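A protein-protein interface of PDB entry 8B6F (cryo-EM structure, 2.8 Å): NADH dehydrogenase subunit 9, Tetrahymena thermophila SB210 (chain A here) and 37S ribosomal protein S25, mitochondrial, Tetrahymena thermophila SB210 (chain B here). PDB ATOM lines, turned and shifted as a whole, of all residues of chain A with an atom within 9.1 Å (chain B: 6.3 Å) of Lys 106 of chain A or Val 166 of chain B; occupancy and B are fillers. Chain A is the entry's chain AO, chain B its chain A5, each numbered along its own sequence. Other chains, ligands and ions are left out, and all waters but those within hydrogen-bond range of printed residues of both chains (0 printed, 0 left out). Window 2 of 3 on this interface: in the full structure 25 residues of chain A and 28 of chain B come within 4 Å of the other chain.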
ATOM      1  N   ASN A   3      18.461  16.112   6.880  1.00  0.00           N
ATOM      2  CA  ASN A   3      18.621  16.959   5.710  1.00  0.00           C
ATOM      3  C   ASN A   3      17.588  18.073   5.772  1.00  0.00           C
ATOM      4  O   ASN A   3      16.658  18.044   6.581  1.00  0.00           O
ATOM      5  CB  ASN A   3      18.470  16.167   4.408  1.00  0.00           C
ATOM      6  CG  ASN A   3      17.066  15.628   4.216  1.00  0.00           C
ATOM      7  OD1 ASN A   3      16.443  15.133   5.154  1.00  0.00           O
ATOM      8  ND2 ASN A   3      16.555  15.733   2.995  1.00  0.00           N
ATOM      9  N   LYS A   4      17.758  19.064   4.902  1.00  0.00           N
ATOM     10  CA  LYS A   4      16.833  20.185   4.814  1.00  0.00           C
ATOM     11  C   LYS A   4      15.743  19.844   3.807  1.00  0.00           C
ATOM     12  O   LYS A   4      16.021  19.673   2.616  1.00  0.00           O
ATOM     13  CB  LYS A   4      17.572  21.462   4.415  1.00  0.00           C
ATOM     14  CG  LYS A   4      18.703  21.821   5.365  1.00  0.00           C
ATOM     15  CD  LYS A   4      19.523  22.989   4.855  1.00  0.00           C
ATOM     16  CE  LYS A   4      20.792  23.159   5.677  1.00  0.00           C
ATOM     17  NZ  LYS A   4      21.701  24.190   5.104  1.00  0.00           N
ATOM     18  N   TYR A   5      14.508  19.735   4.290  1.00  0.00           N
ATOM     19  CA  TYR A   5      13.373  19.317   3.481  1.00  0.00           C
ATOM     20  C   TYR A   5      12.234  20.309   3.645  1.00  0.00           C
ATOM     21  O   TYR A   5      12.034  20.866   4.728  1.00  0.00           O
ATOM     22  CB  TYR A   5      12.906  17.912   3.883  1.00  0.00           C
ATOM     23  CG  TYR A   5      11.545  17.540   3.346  1.00  0.00           C
ATOM     24  CD1 TYR A   5      11.402  16.973   2.086  1.00  0.00           C
ATOM     25  CD2 TYR A   5      10.399  17.753   4.103  1.00  0.00           C
ATOM     26  CE1 TYR A   5      10.157  16.631   1.594  1.00  0.00           C
ATOM     27  CE2 TYR A   5       9.152  17.414   3.620  1.00  0.00           C
ATOM     28  CZ  TYR A   5       9.037  16.854   2.366  1.00  0.00           C
ATOM     29  OH  TYR A   5       7.795  16.517   1.884  1.00  0.00           O
ATOM     30  N   MET A   6      11.492  20.530   2.562  1.00  0.00           N
ATOM     31  CA  MET A   6      10.312  21.380   2.584  1.00  0.00           C
ATOM     32  C   MET A   6       9.209  20.719   1.774  1.00  0.00           C
ATOM     33  O   MET A   6       9.466  20.158   0.705  1.00  0.00           O
ATOM     34  CB  MET A   6      10.610  22.774   2.019  1.00  0.00           C
ATOM     35  CG  MET A   6       9.419  23.717   2.079  1.00  0.00           C
ATOM     36  SD  MET A   6       9.797  25.361   1.454  1.00  0.00           S
ATOM     37  CE  MET A   6       8.204  26.159   1.635  1.00  0.00           C
ATOM     38  N   ASN A  29      13.500   7.853   0.053  1.00  0.00           N
ATOM     39  CA  ASN A  29      14.655   8.716   0.229  1.00  0.00           C
ATOM     40  C   ASN A  29      14.283   9.927   1.079  1.00  0.00           C
ATOM     41  O   ASN A  29      13.108  10.272   1.238  1.00  0.00           O
ATOM     42  CB  ASN A  29      15.207   9.163  -1.124  1.00  0.00           C
ATOM     43  CG  ASN A  29      15.769   8.012  -1.928  1.00  0.00           C
ATOM     44  OD1 ASN A  29      15.347   7.763  -3.056  1.00  0.00           O
ATOM     45  ND2 ASN A  29      16.725   7.297  -1.349  1.00  0.00           N
ATOM     46  N   SER A  30      15.306  10.573   1.637  1.00  0.00           N
ATOM     47  CA  SER A  30      15.065  11.687   2.547  1.00  0.00           C
ATOM     48  C   SER A  30      14.318  12.823   1.863  1.00  0.00           C
ATOM     49  O   SER A  30      13.570  13.555   2.520  1.00  0.00           O
ATOM     50  CB  SER A  30      16.391  12.198   3.112  1.00  0.00           C
ATOM     51  OG  SER A  30      17.113  11.158   3.749  1.00  0.00           O
ATOM     52  N   ASN A  31      14.499  12.983   0.553  1.00  0.00           N
ATOM     53  CA  ASN A  31      13.932  14.097  -0.194  1.00  0.00           C
ATOM     54  C   ASN A  31      12.718  13.696  -1.024  1.00  0.00           C
ATOM     55  O   ASN A  31      12.423  14.350  -2.028  1.00  0.00           O
ATOM     56  CB  ASN A  31      14.998  14.712  -1.100  1.00  0.00           C
ATOM     57  CG  ASN A  31      15.499  13.740  -2.147  1.00  0.00           C
ATOM     58  OD1 ASN A  31      15.617  12.543  -1.892  1.00  0.00           O
ATOM     59  ND2 ASN A  31      15.793  14.250  -3.334  1.00  0.00           N
ATOM     60  N   HIS A  32      12.017  12.636  -0.634  1.00  0.00           N
ATOM     61  CA  HIS A  32      10.915  12.090  -1.412  1.00  0.00           C
ATOM     62  C   HIS A  32       9.607  12.343  -0.677  1.00  0.00           C
ATOM     63  O   HIS A  32       9.501  12.060   0.521  1.00  0.00           O
ATOM     64  CB  HIS A  32      11.117  10.592  -1.649  1.00  0.00           C
ATOM     65  CG  HIS A  32      10.268  10.034  -2.747  1.00  0.00           C
ATOM     66  ND1 HIS A  32       9.125  10.659  -3.196  1.00  0.00           N
ATOM     67  CD2 HIS A  32      10.403   8.913  -3.494  1.00  0.00           C
ATOM     68  CE1 HIS A  32       8.588   9.943  -4.167  1.00  0.00           C
ATOM     69  NE2 HIS A  32       9.344   8.879  -4.368  1.00  0.00           N
ATOM     70  N   SER A  33       8.618  12.874  -1.394  1.00  0.00           N
ATOM     71  CA  SER A  33       7.324  13.212  -0.821  1.00  0.00           C
ATOM     72  C   SER A  33       6.204  12.695  -1.710  1.00  0.00           C
ATOM     73  O   SER A  33       6.248  12.848  -2.933  1.00  0.00           O
ATOM     74  CB  SER A  33       7.182  14.725  -0.643  1.00  0.00           C
ATOM     75  OG  SER A  33       5.926  15.053  -0.075  1.00  0.00           O
ATOM     76  N   LEU A  54      10.400  27.139  -9.833  1.00  0.00           N
ATOM     77  CA  LEU A  54      11.190  26.138  -9.123  1.00  0.00           C
ATOM     78  C   LEU A  54      10.863  24.726  -9.588  1.00  0.00           C
ATOM     79  O   LEU A  54      11.709  23.830  -9.477  1.00  0.00           O
ATOM     80  CB  LEU A  54      10.977  26.271  -7.617  1.00  0.00           C
ATOM     81  CG  LEU A  54      11.429  27.601  -7.003  1.00  0.00           C
ATOM     82  CD1 LEU A  54      11.296  27.550  -5.500  1.00  0.00           C
ATOM     83  CD2 LEU A  54      12.858  27.963  -7.390  1.00  0.00           C
ATOM     84  N   PHE A  55       9.660  24.504 -10.107  1.00  0.00           N
ATOM     85  CA  PHE A  55       9.294  23.211 -10.666  1.00  0.00           C
ATOM     86  C   PHE A  55       9.595  23.108 -12.152  1.00  0.00           C
ATOM     87  O   PHE A  55       9.287  22.081 -12.761  1.00  0.00           O
ATOM     88  CB  PHE A  55       7.809  22.923 -10.430  1.00  0.00           C
ATOM     89  CG  PHE A  55       7.465  22.639  -8.999  1.00  0.00           C
ATOM     90  CD1 PHE A  55       7.880  21.464  -8.396  1.00  0.00           C
ATOM     91  CD2 PHE A  55       6.712  23.536  -8.263  1.00  0.00           C
ATOM     92  CE1 PHE A  55       7.561  21.194  -7.081  1.00  0.00           C
ATOM     93  CE2 PHE A  55       6.389  23.271  -6.948  1.00  0.00           C
ATOM     94  CZ  PHE A  55       6.814  22.098  -6.355  1.00  0.00           C
ATOM     95  N   ASN A  57      12.522  22.807 -13.608  1.00  0.00           N
ATOM     96  CA  ASN A  57      13.535  21.768 -13.780  1.00  0.00           C
ATOM     97  C   ASN A  57      13.046  20.442 -13.195  1.00  0.00           C
ATOM     98  O   ASN A  57      13.642  19.865 -12.289  1.00  0.00           O
ATOM     99  CB  ASN A  57      14.849  22.200 -13.146  1.00  0.00           C
ATOM    100  CG  ASN A  57      15.542  23.286 -13.932  1.00  0.00           C
ATOM    101  OD1 ASN A  57      14.909  24.016 -14.693  1.00  0.00           O
ATOM    102  ND2 ASN A  57      16.853  23.394 -13.765  1.00  0.00           N
ATOM    103  N   TYR A 100       8.111  12.250 -10.200  1.00  0.00           N
ATOM    104  CA  TYR A 100       8.959  13.246 -10.835  1.00  0.00           C
ATOM    105  C   TYR A 100      10.145  13.571  -9.937  1.00  0.00           C
ATOM    106  O   TYR A 100      10.117  13.349  -8.725  1.00  0.00           O
ATOM    107  CB  TYR A 100       8.190  14.543 -11.130  1.00  0.00           C
ATOM    108  CG  TYR A 100       6.765  14.359 -11.600  1.00  0.00           C
ATOM    109  CD1 TYR A 100       5.749  14.067 -10.703  1.00  0.00           C
ATOM    110  CD2 TYR A 100       6.432  14.522 -12.937  1.00  0.00           C
ATOM    111  CE1 TYR A 100       4.446  13.915 -11.126  1.00  0.00           C
ATOM    112  CE2 TYR A 100       5.132  14.372 -13.370  1.00  0.00           C
ATOM    113  CZ  TYR A 100       4.144  14.069 -12.460  1.00  0.00           C
ATOM    114  OH  TYR A 100       2.846  13.921 -12.886  1.00  0.00           O
ATOM    115  N   TYR A 101      11.194  14.105 -10.557  1.00  0.00           N
ATOM    116  CA  TYR A 101      12.371  14.597  -9.856  1.00  0.00           C
ATOM    117  C   TYR A 101      12.614  16.045 -10.254  1.00  0.00           C
ATOM    118  O   TYR A 101      12.627  16.372 -11.444  1.00  0.00           O
ATOM    119  CB  TYR A 101      13.603  13.748 -10.168  1.00  0.00           C
ATOM    120  CG  TYR A 101      14.858  14.268  -9.510  1.00  0.00           C
ATOM    121  CD1 TYR A 101      15.121  14.003  -8.174  1.00  0.00           C
ATOM    122  CD2 TYR A 101      15.776  15.023 -10.223  1.00  0.00           C
ATOM    123  CE1 TYR A 101      16.261  14.477  -7.565  1.00  0.00           C
ATOM    124  CE2 TYR A 101      16.921  15.502  -9.622  1.00  0.00           C
ATOM    125  CZ  TYR A 101      17.158  15.224  -8.293  1.00  0.00           C
ATOM    126  OH  TYR A 101      18.298  15.700  -7.690  1.00  0.00           O
ATOM    127  N   ASN A 102      12.811  16.901  -9.256  1.00  0.00           N
ATOM    128  CA  ASN A 102      13.062  18.323  -9.448  1.00  0.00           C
ATOM    129  C   ASN A 102      14.501  18.636  -9.067  1.00  0.00           C
ATOM    130  O   ASN A 102      14.952  18.272  -7.978  1.00  0.00           O
ATOM    131  CB  ASN A 102      12.095  19.159  -8.608  1.00  0.00           C
ATOM    132  CG  ASN A 102      12.241  20.645  -8.856  1.00  0.00           C
ATOM    133  OD1 ASN A 102      13.216  21.095  -9.453  1.00  0.00           O
ATOM    134  ND2 ASN A 102      11.270  21.417  -8.389  1.00  0.00           N
ATOM    135  N   TYR A 103      15.216  19.319  -9.965  1.00  0.00           N
ATOM    136  CA  TYR A 103      16.638  19.574  -9.759  1.00  0.00           C
ATOM    137  C   TYR A 103      16.880  20.807  -8.899  1.00  0.00           C
ATOM    138  O   TYR A 103      17.801  20.816  -8.076  1.00  0.00           O
ATOM    139  CB  TYR A 103      17.344  19.729 -11.105  1.00  0.00           C
ATOM    140  CG  TYR A 103      17.473  18.439 -11.878  1.00  0.00           C
ATOM    141  CD1 TYR A 103      16.446  17.988 -12.695  1.00  0.00           C
ATOM    142  CD2 TYR A 103      18.628  17.678 -11.799  1.00  0.00           C
ATOM    143  CE1 TYR A 103      16.564  16.809 -13.404  1.00  0.00           C
ATOM    144  CE2 TYR A 103      18.758  16.500 -12.504  1.00  0.00           C
ATOM    145  CZ  TYR A 103      17.722  16.071 -13.305  1.00  0.00           C
ATOM    146  OH  TYR A 103      17.849  14.897 -14.008  1.00  0.00           O
ATOM    147  N   PHE A 104      16.087  21.863  -9.082  1.00  0.00           N
ATOM    148  CA  PHE A 104      16.279  23.061  -8.275  1.00  0.00           C
ATOM    149  C   PHE A 104      16.104  22.763  -6.794  1.00  0.00           C
ATOM    150  O   PHE A 104      16.901  23.214  -5.964  1.00  0.00           O
ATOM    151  CB  PHE A 104      15.296  24.154  -8.699  1.00  0.00           C
ATOM    152  CG  PHE A 104      15.725  24.934  -9.907  1.00  0.00           C
ATOM    153  CD1 PHE A 104      17.053  25.274 -10.114  1.00  0.00           C
ATOM    154  CD2 PHE A 104      14.784  25.351 -10.825  1.00  0.00           C
ATOM    155  CE1 PHE A 104      17.431  25.998 -11.221  1.00  0.00           C
ATOM    156  CE2 PHE A 104      15.154  26.074 -11.928  1.00  0.00           C
ATOM    157  CZ  PHE A 104      16.480  26.401 -12.130  1.00  0.00           C
ATOM    158  N   LEU A 105      15.069  22.006  -6.441  1.00  0.00           N
ATOM    159  CA  LEU A 105      14.801  21.666  -5.052  1.00  0.00           C
ATOM    160  C   LEU A 105      15.425  20.345  -4.630  1.00  0.00           C
ATOM    161  O   LEU A 105      15.289  19.961  -3.464  1.00  0.00           O
ATOM    162  CB  LEU A 105      13.288  21.612  -4.817  1.00  0.00           C
ATOM    163  CG  LEU A 105      12.512  22.862  -5.234  1.00  0.00           C
ATOM    164  CD1 LEU A 105      11.024  22.667  -5.010  1.00  0.00           C
ATOM    165  CD2 LEU A 105      13.008  24.082  -4.483  1.00  0.00           C
ATOM    166  N   LYS A 106      16.101  19.646  -5.536  1.00  0.00           N
ATOM    167  CA  LYS A 106      16.735  18.368  -5.226  1.00  0.00           C
ATOM    168  C   LYS A 106      15.744  17.426  -4.549  1.00  0.00           C
ATOM    169  O   LYS A 106      16.025  16.833  -3.506  1.00  0.00           O
ATOM    170  CB  LYS A 106      17.970  18.571  -4.345  1.00  0.00           C
ATOM    171  CG  LYS A 106      18.980  19.580  -4.873  1.00  0.00           C
ATOM    172  CD  LYS A 106      19.659  19.096  -6.140  1.00  0.00           C
ATOM    173  CE  LYS A 106      20.711  20.091  -6.606  1.00  0.00           C
ATOM    174  NZ  LYS A 106      21.361  19.663  -7.873  1.00  0.00           N
ATOM    175  N   SER A 107      14.564  17.292  -5.147  1.00  0.00           N
ATOM    176  CA  SER A 107      13.448  16.616  -4.504  1.00  0.00           C
ATOM    177  C   SER A 107      12.837  15.592  -5.448  1.00  0.00           C
ATOM    178  O   SER A 107      12.997  15.660  -6.668  1.00  0.00           O
ATOM    179  CB  SER A 107      12.373  17.613  -4.054  1.00  0.00           C
ATOM    180  OG  SER A 107      11.797  18.277  -5.164  1.00  0.00           O
ATOM    181  N   LYS A 108      12.124  14.638  -4.853  1.00  0.00           N
ATOM    182  CA  LYS A 108      11.322  13.662  -5.575  1.00  0.00           C
ATOM    183  C   LYS A 108       9.874  13.824  -5.144  1.00  0.00           C
ATOM    184  O   LYS A 108       9.583  13.874  -3.945  1.00  0.00           O
ATOM    185  CB  LYS A 108      11.794  12.233  -5.303  1.00  0.00           C
ATOM    186  CG  LYS A 108      13.226  11.951  -5.712  1.00  0.00           C
ATOM    187  CD  LYS A 108      13.614  10.523  -5.369  1.00  0.00           C
ATOM    188  CE  LYS A 108      15.037  10.220  -5.799  1.00  0.00           C
ATOM    189  NZ  LYS A 108      15.424   8.816  -5.489  1.00  0.00           N
ATOM    190  N   LEU A 109       8.972  13.910  -6.117  1.00  0.00           N
ATOM    191  CA  LEU A 109       7.557  14.145  -5.859  1.00  0.00           C
ATOM    192  C   LEU A 109       6.746  13.067  -6.559  1.00  0.00           C
ATOM    193  O   LEU A 109       6.823  12.929  -7.783  1.00  0.00           O
ATOM    194  CB  LEU A 109       7.139  15.534  -6.346  1.00  0.00           C
ATOM    195  CG  LEU A 109       5.644  15.857  -6.321  1.00  0.00           C
ATOM    196  CD1 LEU A 109       5.099  15.775  -4.906  1.00  0.00           C
ATOM    197  CD2 LEU A 109       5.390  17.228  -6.918  1.00  0.00           C
ATOM    198  N   PHE B 154      14.748  27.768   1.560  1.00  0.00           N
ATOM    199  CA  PHE B 154      14.995  26.352   1.316  1.00  0.00           C
ATOM    200  C   PHE B 154      15.748  26.144   0.012  1.00  0.00           C
ATOM    201  O   PHE B 154      16.671  25.325  -0.057  1.00  0.00           O
ATOM    202  CB  PHE B 154      13.676  25.581   1.298  1.00  0.00           C
ATOM    203  CG  PHE B 154      13.805  24.179   0.785  1.00  0.00           C
ATOM    204  CD1 PHE B 154      14.236  23.159   1.617  1.00  0.00           C
ATOM    205  CD2 PHE B 154      13.494  23.877  -0.529  1.00  0.00           C
ATOM    206  CE1 PHE B 154      14.357  21.867   1.146  1.00  0.00           C
ATOM    207  CE2 PHE B 154      13.614  22.587  -1.007  1.00  0.00           C
ATOM    208  CZ  PHE B 154      14.046  21.580  -0.167  1.00  0.00           C
ATOM    209  N   VAL B 158      19.213  24.116   0.510  1.00  0.00           N
ATOM    210  CA  VAL B 158      19.307  22.742   0.024  1.00  0.00           C
ATOM    211  C   VAL B 158      20.462  22.605  -0.960  1.00  0.00           C
ATOM    212  O   VAL B 158      21.206  21.617  -0.935  1.00  0.00           O
ATOM    213  CB  VAL B 158      17.970  22.293  -0.598  1.00  0.00           C
ATOM    214  CG1 VAL B 158      17.660  23.068  -1.873  1.00  0.00           C
ATOM    215  CG2 VAL B 158      17.993  20.797  -0.875  1.00  0.00           C
ATOM    216  N   ASN B 159      20.623  23.586  -1.847  1.00  0.00           N
ATOM    217  CA  ASN B 159      21.758  23.578  -2.761  1.00  0.00           C
ATOM    218  C   ASN B 159      23.066  23.822  -2.021  1.00  0.00           C
ATOM    219  O   ASN B 159      24.102  23.251  -2.376  1.00  0.00           O
ATOM    220  CB  ASN B 159      21.555  24.627  -3.852  1.00  0.00           C
ATOM    221  CG  ASN B 159      20.414  24.280  -4.785  1.00  0.00           C
ATOM    222  OD1 ASN B 159      20.614  23.631  -5.811  1.00  0.00           O
ATOM    223  ND2 ASN B 159      19.210  24.713  -4.434  1.00  0.00           N
ATOM    224  N   ALA B 160      23.041  24.662  -0.986  1.00  0.00           N
ATOM    225  CA  ALA B 160      24.262  24.929  -0.236  1.00  0.00           C
ATOM    226  C   ALA B 160      24.791  23.666   0.432  1.00  0.00           C
ATOM    227  O   ALA B 160      26.003  23.421   0.437  1.00  0.00           O
ATOM    228  CB  ALA B 160      24.007  26.018   0.804  1.00  0.00           C
ATOM    229  N   GLU B 161      23.903  22.850   1.000  1.00  0.00           N
ATOM    230  CA  GLU B 161      24.343  21.679   1.749  1.00  0.00           C
ATOM    231  C   GLU B 161      24.869  20.558   0.860  1.00  0.00           C
ATOM    232  O   GLU B 161      25.424  19.588   1.388  1.00  0.00           O
ATOM    233  CB  GLU B 161      23.201  21.147   2.619  1.00  0.00           C
ATOM    234  CG  GLU B 161      21.994  20.648   1.841  1.00  0.00           C
ATOM    235  CD  GLU B 161      20.982  19.952   2.730  1.00  0.00           C
ATOM    236  OE1 GLU B 161      21.263  19.791   3.936  1.00  0.00           O
ATOM    237  OE2 GLU B 161      19.907  19.566   2.226  1.00  0.00           O
ATOM    238  N   GLU B 162      24.705  20.650  -0.457  1.00  0.00           N
ATOM    239  CA  GLU B 162      25.203  19.607  -1.343  1.00  0.00           C
ATOM    240  C   GLU B 162      26.726  19.638  -1.413  1.00  0.00           C
ATOM    241  O   GLU B 162      27.355  20.696  -1.331  1.00  0.00           O
ATOM    242  CB  GLU B 162      24.616  19.770  -2.745  1.00  0.00           C
ATOM    243  CG  GLU B 162      23.114  19.550  -2.813  1.00  0.00           C
ATOM    244  CD  GLU B 162      22.705  18.144  -2.417  1.00  0.00           C
ATOM    245  OE1 GLU B 162      23.579  17.254  -2.387  1.00  0.00           O
ATOM    246  OE2 GLU B 162      21.509  17.928  -2.131  1.00  0.00           O
ATOM    247  N   VAL B 163      27.318  18.456  -1.581  1.00  0.00           N
ATOM    248  CA  VAL B 163      28.768  18.302  -1.544  1.00  0.00           C
ATOM    249  C   VAL B 163      29.339  18.250  -2.955  1.00  0.00           C
ATOM    250  O   VAL B 163      30.450  18.728  -3.202  1.00  0.00           O
ATOM    251  CB  VAL B 163      29.167  17.044  -0.752  1.00  0.00           C
ATOM    252  CG1 VAL B 163      30.678  16.905  -0.692  1.00  0.00           C
ATOM    253  CG2 VAL B 163      28.584  17.090   0.645  1.00  0.00           C
ATOM    254  N   TRP B 164      28.597  17.655  -3.886  1.00  0.00           N
ATOM    255  CA  TRP B 164      29.104  17.442  -5.236  1.00  0.00           C
ATOM    256  C   TRP B 164      28.137  17.970  -6.287  1.00  0.00           C
ATOM    257  O   TRP B 164      28.559  18.384  -7.372  1.00  0.00           O
ATOM    258  CB  TRP B 164      29.373  15.950  -5.457  1.00  0.00           C
ATOM    259  CG  TRP B 164      29.675  15.587  -6.875  1.00  0.00           C
ATOM    260  CD1 TRP B 164      30.905  15.447  -7.439  1.00  0.00           C
ATOM    261  CD2 TRP B 164      28.724  15.309  -7.909  1.00  0.00           C
ATOM    262  NE1 TRP B 164      30.782  15.103  -8.763  1.00  0.00           N
ATOM    263  CE2 TRP B 164      29.452  15.013  -9.076  1.00  0.00           C
ATOM    264  CE3 TRP B 164      27.326  15.287  -7.962  1.00  0.00           C
ATOM    265  CZ2 TRP B 164      28.829  14.698 -10.282  1.00  0.00           C
ATOM    266  CZ3 TRP B 164      26.711  14.974  -9.158  1.00  0.00           C
ATOM    267  CH2 TRP B 164      27.462  14.683 -10.303  1.00  0.00           C
ATOM    268  N   SER B 165      26.840  17.966  -5.976  1.00  0.00           N
ATOM    269  CA  SER B 165      25.839  18.300  -6.986  1.00  0.00           C
ATOM    270  C   SER B 165      26.001  19.730  -7.489  1.00  0.00           C
ATOM    271  O   SER B 165      25.904  19.982  -8.694  1.00  0.00           O
ATOM    272  CB  SER B 165      24.435  18.093  -6.417  1.00  0.00           C
ATOM    273  OG  SER B 165      24.204  16.730  -6.107  1.00  0.00           O
ATOM    274  N   VAL B 166      26.243  20.677  -6.586  1.00  0.00           N
ATOM    275  CA  VAL B 166      26.328  22.090  -6.939  1.00  0.00           C
ATOM    276  C   VAL B 166      27.536  22.698  -6.245  1.00  0.00           C
ATOM    277  O   VAL B 166      27.818  22.391  -5.082  1.00  0.00           O
ATOM    278  CB  VAL B 166      25.039  22.851  -6.562  1.00  0.00           C
ATOM    279  CG1 VAL B 166      23.817  22.140  -7.120  1.00  0.00           C
ATOM    280  CG2 VAL B 166      24.925  23.011  -5.058  1.00  0.00           C
ATOM    281  N   SER B 167      28.254  23.558  -6.963  1.00  0.00           N
ATOM    282  CA  SER B 167      29.413  24.240  -6.395  1.00  0.00           C
ATOM    283  C   SER B 167      29.683  25.487  -7.225  1.00  0.00           C
ATOM    284  O   SER B 167      30.081  25.379  -8.388  1.00  0.00           O
ATOM    285  CB  SER B 167      30.625  23.317  -6.373  1.00  0.00           C
ATOM    286  OG  SER B 167      31.761  23.979  -5.848  1.00  0.00           O
ATOM    287  N   ILE B 168      29.469  26.662  -6.627  1.00  0.00           N
ATOM    288  CA  ILE B 168      29.748  27.914  -7.323  1.00  0.00           C
ATOM    289  C   ILE B 168      31.237  28.045  -7.608  1.00  0.00           C
ATOM    290  O   ILE B 168      31.635  28.606  -8.635  1.00  0.00           O
ATOM    291  CB  ILE B 168      29.214  29.110  -6.510  1.00  0.00           C
ATOM    292  CG1 ILE B 168      29.230  30.388  -7.355  1.00  0.00           C
ATOM    293  CG2 ILE B 168      30.029  29.315  -5.240  1.00  0.00           C
ATOM    294  CD1 ILE B 168      28.245  30.382  -8.507  1.00  0.00           C
ATOM    295  N   GLU B 170      33.207  25.558  -8.370  1.00  0.00           N
ATOM    296  CA  GLU B 170      33.401  24.777  -9.586  1.00  0.00           C
ATOM    297  C   GLU B 170      32.888  25.532 -10.804  1.00  0.00           C
ATOM    298  O   GLU B 170      33.504  25.487 -11.875  1.00  0.00           O
ATOM    299  CB  GLU B 170      32.697  23.426  -9.456  1.00  0.00           C
ATOM    300  CG  GLU B 170      32.746  22.561 -10.713  1.00  0.00           C
ATOM    301  CD  GLU B 170      34.162  22.227 -11.145  1.00  0.00           C
ATOM    302  OE1 GLU B 170      35.098  22.450 -10.349  1.00  0.00           O
ATOM    303  OE2 GLU B 170      34.339  21.737 -12.282  1.00  0.00           O
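Of chain B, only Asn 159 (3.6 Å), Ser 165 (3.7 Å) and Val 166 (3.6 Å) come within 4 Å of Lys 106 of chain A. Printed residues of chain A within 4 Å of Phe 154 of chain B: Lys 4 (3.1 Å), Tyr 5 (3.6 Å), Met 6 (3.5 Å) and Leu 105 (3.8 Å). Printed residues of chain A within 4 Å of Asn 159 of chain B: Phe 104 and Lys 106. Of the printed residues of chain A, Glu 161 of chain B touches Lys 4 (3.5 Å). Of the printed residues of chain A, Ser 165 of chain B touches Lys 106 (3.7 Å). Val 166 of chain B touches just one residue of chain A: Lys 106 (3.6 Å). The nearest residue of chain B that does not touch Lys 106 of chain A is Glu 162 of chain B (4.1 Å). The nearest residue of chain A that does not touch Val 166 of chain B is Tyr 103 of chain A (6.2 Å).
OE2 of Glu 161 of chain B lies within hydrogen-bond range of N of Lys 4 of chain A (3.5 Å). The side-chain amide nitrogen (ND2) of Asn 159 of chain B is in hydrogen-bond range of the backbone carbonyl oxygen (O) of Phe 104 of chain A (3.1 Å).
Printed residues of chain A that touch a printed residue of chain B: Lys 4, Tyr 5, Met 6, Phe 104, Leu 105 and Lys 106. Hydrophobic or aromatic side chains of chain A within 4 Å of the printed part of chain B: Met 6 and Leu 105. Among the printed residues, 10 pairs touch across the chains. Among the printed residues, no Asp or Glu carboxylate lies within 4 Å of a Lys or Arg side-chain nitrogen of the other chain.
O of Lys 4 of chain A touches CE1 of Phe 154 of chain B (3.1 Å). CE1 of Phe 154 of chain B touches CA of Tyr 5 of chain A, at 3.6 Å. N of Met 6 of chain A touches CE1 of Phe 154 of chain B, 3.5 Å away. Leu 105 of chain A touches Phe 154 of chain B. Val 158 of chain B touches Leu 105 of chain A. Lys 106 of chain A touches Asn 159 of chain B. Ser 165 of chain B touches Lys 106 of chain A (CB to NZ, 3.7 Å). CG1 of Val 166 of chain B touches NZ of Lys 106 of chain A (3.6 Å).
The side-chain hydroxyl (OH) of Tyr 5 of chain A sits at hydrogen-bond distance from the side-chain hydroxyl (OG) of Ser 33 of chain A (3.1 Å). The backbone carbonyl oxygen (O) of Lys 106 of chain A is in hydrogen-bond range of the side-chain amide nitrogen (ND2) of Asn 31 of chain A (2.6 Å). The backbone NH of Phe 104 of chain A sits at hydrogen-bond distance from the side-chain amide oxygen of Asn 102 of chain A.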
